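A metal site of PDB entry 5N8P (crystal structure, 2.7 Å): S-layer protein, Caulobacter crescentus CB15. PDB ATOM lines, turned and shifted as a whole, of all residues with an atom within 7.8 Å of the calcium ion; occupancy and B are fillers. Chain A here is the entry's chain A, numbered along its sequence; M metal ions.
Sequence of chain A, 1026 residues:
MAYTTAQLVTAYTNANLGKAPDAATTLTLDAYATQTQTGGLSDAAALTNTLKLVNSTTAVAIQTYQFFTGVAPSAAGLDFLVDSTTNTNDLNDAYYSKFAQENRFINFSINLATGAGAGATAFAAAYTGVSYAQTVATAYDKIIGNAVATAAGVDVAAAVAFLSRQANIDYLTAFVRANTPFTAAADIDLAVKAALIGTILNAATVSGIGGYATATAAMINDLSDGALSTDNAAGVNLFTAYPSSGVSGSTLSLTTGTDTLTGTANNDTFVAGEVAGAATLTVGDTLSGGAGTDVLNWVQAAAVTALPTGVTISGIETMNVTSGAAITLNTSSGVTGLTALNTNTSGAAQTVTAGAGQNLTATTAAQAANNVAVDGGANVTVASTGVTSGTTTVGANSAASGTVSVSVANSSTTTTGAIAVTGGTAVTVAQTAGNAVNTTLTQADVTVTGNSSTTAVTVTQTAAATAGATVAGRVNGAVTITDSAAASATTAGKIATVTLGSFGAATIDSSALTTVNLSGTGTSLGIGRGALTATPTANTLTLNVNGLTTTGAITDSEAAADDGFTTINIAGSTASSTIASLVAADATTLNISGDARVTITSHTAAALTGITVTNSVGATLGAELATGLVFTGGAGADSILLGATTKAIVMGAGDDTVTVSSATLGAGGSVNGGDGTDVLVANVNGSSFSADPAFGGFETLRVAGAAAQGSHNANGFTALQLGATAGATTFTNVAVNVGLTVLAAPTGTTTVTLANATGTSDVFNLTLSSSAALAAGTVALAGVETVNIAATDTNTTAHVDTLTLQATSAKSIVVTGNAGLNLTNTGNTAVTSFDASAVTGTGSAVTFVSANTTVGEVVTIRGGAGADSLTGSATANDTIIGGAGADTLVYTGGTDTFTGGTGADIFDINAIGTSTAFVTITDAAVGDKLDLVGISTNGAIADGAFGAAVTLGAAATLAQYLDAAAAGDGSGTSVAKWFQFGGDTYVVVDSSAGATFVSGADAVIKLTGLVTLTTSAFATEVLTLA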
ATOM      1  N   SER A 253      -2.998  -9.427  -5.370  1.00  0.00           N
ATOM      2  CA  SER A 253      -3.472  -9.035  -6.684  1.00  0.00           C
ATOM      3  C   SER A 253      -2.704  -7.893  -7.354  1.00  0.00           C
ATOM      4  O   SER A 253      -2.665  -6.802  -6.812  1.00  0.00           O
ATOM      5  CB  SER A 253      -4.920  -8.605  -6.576  1.00  0.00           C
ATOM      6  OG  SER A 253      -5.736  -9.724  -6.713  1.00  0.00           O
ATOM      7  N   LEU A 254      -2.197  -8.147  -8.565  1.00  0.00           N
ATOM      8  CA  LEU A 254      -1.590  -7.099  -9.387  1.00  0.00           C
ATOM      9  C   LEU A 254      -2.652  -6.187  -9.972  1.00  0.00           C
ATOM     10  O   LEU A 254      -3.766  -6.627 -10.186  1.00  0.00           O
ATOM     11  CB  LEU A 254      -0.756  -7.698 -10.519  1.00  0.00           C
ATOM     12  CG  LEU A 254       0.716  -8.059 -10.234  1.00  0.00           C
ATOM     13  CD1 LEU A 254       0.822  -9.308  -9.401  1.00  0.00           C
ATOM     14  CD2 LEU A 254       1.469  -8.268 -11.536  1.00  0.00           C
ATOM     15  N   THR A 255      -2.318  -4.912 -10.213  1.00  0.00           N
ATOM     16  CA  THR A 255      -3.218  -3.911 -10.821  1.00  0.00           C
ATOM     17  C   THR A 255      -2.715  -3.433 -12.165  1.00  0.00           C
ATOM     18  O   THR A 255      -1.607  -3.784 -12.549  1.00  0.00           O
ATOM     19  CB  THR A 255      -3.362  -2.663  -9.955  1.00  0.00           C
ATOM     20  OG1 THR A 255      -2.193  -1.851 -10.137  1.00  0.00           O
ATOM     21  CG2 THR A 255      -3.535  -3.051  -8.473  1.00  0.00           C
ATOM     22  N   THR A 256      -3.468  -2.603 -12.869  1.00  0.00           N
ATOM     23  CA  THR A 256      -2.963  -2.097 -14.158  1.00  0.00           C
ATOM     24  C   THR A 256      -1.817  -1.079 -13.951  1.00  0.00           C
ATOM     25  O   THR A 256      -1.303  -0.534 -14.941  1.00  0.00           O
ATOM     26  CB  THR A 256      -4.052  -1.438 -15.030  1.00  0.00           C
ATOM     27  OG1 THR A 256      -4.578  -0.315 -14.349  1.00  0.00           O
ATOM     28  CG2 THR A 256      -5.207  -2.375 -15.255  1.00  0.00           C
ATOM     29  N   GLY A 257      -1.398  -0.860 -12.708  1.00  0.00           N
ATOM     30  CA  GLY A 257      -0.267   0.031 -12.394  1.00  0.00           C
ATOM     31  C   GLY A 257       1.146  -0.575 -12.235  1.00  0.00           C
ATOM     32  O   GLY A 257       1.477  -1.579 -12.850  1.00  0.00           O
ATOM     33  N   THR A 258       1.976   0.061 -11.413  1.00  0.00           N
ATOM     34  CA  THR A 258       3.225  -0.514 -11.012  1.00  0.00           C
ATOM     35  C   THR A 258       3.118  -1.045  -9.600  1.00  0.00           C
ATOM     36  O   THR A 258       2.924  -0.298  -8.653  1.00  0.00           O
ATOM     37  CB  THR A 258       4.377   0.507 -11.152  1.00  0.00           C
ATOM     38  OG1 THR A 258       4.528   0.804 -12.531  1.00  0.00           O
ATOM     39  CG2 THR A 258       5.673  -0.072 -10.626  1.00  0.00           C
ATOM     40  N   ASP A 259       3.258  -2.373  -9.477  1.00  0.00           N
ATOM     41  CA  ASP A 259       3.042  -3.025  -8.199  1.00  0.00           C
ATOM     42  C   ASP A 259       4.347  -3.392  -7.553  1.00  0.00           C
ATOM     43  O   ASP A 259       5.291  -3.822  -8.210  1.00  0.00           O
ATOM     44  CB  ASP A 259       2.170  -4.247  -8.413  1.00  0.00           C
ATOM     45  CG  ASP A 259       0.877  -3.909  -9.166  1.00  0.00           C
ATOM     46  OD1 ASP A 259      -0.043  -3.273  -8.567  1.00  0.00           O
ATOM     47  OD2 ASP A 259       0.798  -4.212 -10.369  1.00  0.00           O
ATOM     48  N   THR A 260       4.397  -3.232  -6.233  1.00  0.00           N
ATOM     49  CA  THR A 260       5.537  -3.654  -5.438  1.00  0.00           C
ATOM     50  C   THR A 260       5.030  -4.599  -4.341  1.00  0.00           C
ATOM     51  O   THR A 260       4.660  -4.186  -3.241  1.00  0.00           O
ATOM     52  CB  THR A 260       6.355  -2.457  -4.914  1.00  0.00           C
ATOM     53  OG1 THR A 260       6.618  -1.560  -6.012  1.00  0.00           O
ATOM     54  CG2 THR A 260       7.694  -2.919  -4.317  1.00  0.00           C
ATOM     55  N   LEU A 261       5.021  -5.893  -4.651  1.00  0.00           N
ATOM     56  CA  LEU A 261       4.359  -6.881  -3.823  1.00  0.00           C
ATOM     57  C   LEU A 261       5.356  -7.826  -3.191  1.00  0.00           C
ATOM     58  O   LEU A 261       6.285  -8.298  -3.851  1.00  0.00           O
ATOM     59  CB  LEU A 261       3.308  -7.632  -4.629  1.00  0.00           C
ATOM     60  CG  LEU A 261       2.198  -6.816  -5.282  1.00  0.00           C
ATOM     61  CD1 LEU A 261       1.224  -7.678  -6.074  1.00  0.00           C
ATOM     62  CD2 LEU A 261       1.451  -5.903  -4.282  1.00  0.00           C
ATOM     63  N   ALA A 272      -1.990 -12.267 -11.487  1.00  0.00           N
ATOM     64  CA  ALA A 272      -1.737 -11.286 -12.512  1.00  0.00           C
ATOM     65  C   ALA A 272      -2.738 -11.410 -13.647  1.00  0.00           C
ATOM     66  O   ALA A 272      -2.379 -11.593 -14.806  1.00  0.00           O
ATOM     67  CB  ALA A 272      -0.333 -11.399 -13.008  1.00  0.00           C
ATOM     68  N   ALA A 279      -4.437  -5.956 -19.032  1.00  0.00           N
ATOM     69  CA  ALA A 279      -3.392  -6.762 -18.389  1.00  0.00           C
ATOM     70  C   ALA A 279      -2.923  -6.186 -17.052  1.00  0.00           C
ATOM     71  O   ALA A 279      -2.879  -4.948 -16.929  1.00  0.00           O
ATOM     72  CB  ALA A 279      -2.219  -6.886 -19.322  1.00  0.00           C
ATOM     73  N   THR A 280      -2.608  -7.027 -16.072  1.00  0.00           N
ATOM     74  CA  THR A 280      -2.064  -6.488 -14.802  1.00  0.00           C
ATOM     75  C   THR A 280      -0.578  -6.734 -14.534  1.00  0.00           C
ATOM     76  O   THR A 280      -0.015  -6.191 -13.572  1.00  0.00           O
ATOM     77  CB  THR A 280      -2.892  -6.827 -13.544  1.00  0.00           C
ATOM     78  OG1 THR A 280      -2.757  -8.218 -13.215  1.00  0.00           O
ATOM     79  CG2 THR A 280      -4.335  -6.452 -13.730  1.00  0.00           C
ATOM     80  N   LEU A 281       0.070  -7.552 -15.353  1.00  0.00           N
ATOM     81  CA  LEU A 281       1.529  -7.583 -15.347  1.00  0.00           C
ATOM     82  C   LEU A 281       1.989  -6.529 -16.340  1.00  0.00           C
ATOM     83  O   LEU A 281       1.763  -6.646 -17.547  1.00  0.00           O
ATOM     84  CB  LEU A 281       2.095  -8.962 -15.620  1.00  0.00           C
ATOM     85  CG  LEU A 281       3.540  -9.175 -15.208  1.00  0.00           C
ATOM     86  CD1 LEU A 281       3.691  -9.586 -13.756  1.00  0.00           C
ATOM     87  CD2 LEU A 281       4.139 -10.264 -16.068  1.00  0.00           C
ATOM     88  N   THR A 282       2.584  -5.475 -15.803  1.00  0.00           N
ATOM     89  CA  THR A 282       2.851  -4.225 -16.537  1.00  0.00           C
ATOM     90  C   THR A 282       4.177  -3.642 -16.121  1.00  0.00           C
ATOM     91  O   THR A 282       4.800  -4.109 -15.144  1.00  0.00           O
ATOM     92  CB  THR A 282       1.810  -3.173 -16.189  1.00  0.00           C
ATOM     93  OG1 THR A 282       1.553  -3.254 -14.785  1.00  0.00           O
ATOM     94  CG2 THR A 282       0.497  -3.412 -16.947  1.00  0.00           C
ATOM     95  N   VAL A 283       4.597  -2.583 -16.812  1.00  0.00           N
ATOM     96  CA  VAL A 283       5.912  -1.992 -16.607  1.00  0.00           C
ATOM     97  C   VAL A 283       6.266  -1.714 -15.141  1.00  0.00           C
ATOM     98  O   VAL A 283       5.471  -1.178 -14.411  1.00  0.00           O
ATOM     99  CB  VAL A 283       6.223  -0.823 -17.613  1.00  0.00           C
ATOM    100  CG1 VAL A 283       5.283  -0.810 -18.831  1.00  0.00           C
ATOM    101  CG2 VAL A 283       6.030   0.501 -16.985  1.00  0.00           C
ATOM    102  N   GLY A 284       7.456  -2.167 -14.725  1.00  0.00           N
ATOM    103  CA  GLY A 284       8.017  -1.893 -13.403  1.00  0.00           C
ATOM    104  C   GLY A 284       7.544  -2.786 -12.273  1.00  0.00           C
ATOM    105  O   GLY A 284       8.113  -2.698 -11.162  1.00  0.00           O
ATOM    106  N   ASP A 285       6.525  -3.604 -12.522  1.00  0.00           N
ATOM    107  CA  ASP A 285       6.016  -4.548 -11.537  1.00  0.00           C
ATOM    108  C   ASP A 285       7.155  -5.337 -10.884  1.00  0.00           C
ATOM    109  O   ASP A 285       7.924  -6.005 -11.579  1.00  0.00           O
ATOM    110  CB  ASP A 285       5.028  -5.538 -12.171  1.00  0.00           C
ATOM    111  CG  ASP A 285       3.643  -4.962 -12.430  1.00  0.00           C
ATOM    112  OD1 ASP A 285       2.868  -5.611 -13.170  1.00  0.00           O
ATOM    113  OD2 ASP A 285       3.279  -3.882 -11.901  1.00  0.00           O
ATOM    114  N   THR A 286       7.289  -5.266  -9.568  1.00  0.00           N
ATOM    115  CA  THR A 286       8.282  -6.133  -8.925  1.00  0.00           C
ATOM    116  C   THR A 286       7.647  -6.986  -7.838  1.00  0.00           C
ATOM    117  O   THR A 286       6.979  -6.479  -6.926  1.00  0.00           O
ATOM    118  CB  THR A 286       9.582  -5.390  -8.463  1.00  0.00           C
ATOM    119  OG1 THR A 286       9.308  -4.626  -7.297  1.00  0.00           O
ATOM    120  CG2 THR A 286      10.224  -4.472  -9.563  1.00  0.00           C
ATOM    121  N   LEU A 287       7.858  -8.305  -7.969  1.00  0.00           N
ATOM    122  CA  LEU A 287       7.248  -9.304  -7.078  1.00  0.00           C
ATOM    123  C   LEU A 287       8.295 -10.095  -6.321  1.00  0.00           C
ATOM    124  O   LEU A 287       9.327 -10.457  -6.879  1.00  0.00           O
ATOM    125  CB  LEU A 287       6.284 -10.220  -7.848  1.00  0.00           C
ATOM    126  CG  LEU A 287       5.343  -9.604  -8.870  1.00  0.00           C
ATOM    127  CD1 LEU A 287       4.779 -10.656  -9.820  1.00  0.00           C
ATOM    128  CD2 LEU A 287       4.272  -8.776  -8.161  1.00  0.00           C
ATOM    129  N   VAL A 311      10.069  -5.325 -15.125  1.00  0.00           N
ATOM    130  CA  VAL A 311       9.465  -6.421 -14.371  1.00  0.00           C
ATOM    131  C   VAL A 311      10.558  -7.323 -13.819  1.00  0.00           C
ATOM    132  O   VAL A 311      11.478  -7.685 -14.554  1.00  0.00           O
ATOM    133  CB  VAL A 311       8.416  -7.204 -15.202  1.00  0.00           C
ATOM    134  CG1 VAL A 311       7.973  -8.500 -14.489  1.00  0.00           C
ATOM    135  CG2 VAL A 311       7.193  -6.348 -15.466  1.00  0.00           C
HETATM  136 CA    CA M   1       0.862  -4.190 -12.671  1.00  0.00          CA
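The backbone NH of Thr 286 lies within hydrogen-bond range of the backbone carbonyl oxygen of Asp 259 (2.8 Å). The backbone NH (N) of Gly 257 is in hydrogen-bond range of the side-chain hydroxyl (OG1) of Thr 255, at 2.9 Å.
Six residues have an atom within 4 Å of the calcium ion: Thr 255, Gly 257, Asp 259, Thr 280, Thr 282 and Asp 285. The nearest printed residue that does not touch the calcium ion is Leu 254 (4.3 Å).
The calcium ion is bound by the side-chain carboxylate (OD2) of Asp 259 (2.3 Å), the backbone carbonyl oxygen (O) of Thr 280 (2.4 Å), the side-chain hydroxyl (OG1) of Thr 282 (2.4 Å), the backbone carbonyl oxygen (O) of Thr 255 (2.5 Å), the side-chain carboxylate (OD1) of Asp 285 (2.5 Å), the side-chain carboxylate (OD2) of Asp 285 (2.6 Å) and the backbone carbonyl oxygen (O) of Gly 257 (2.7 Å).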
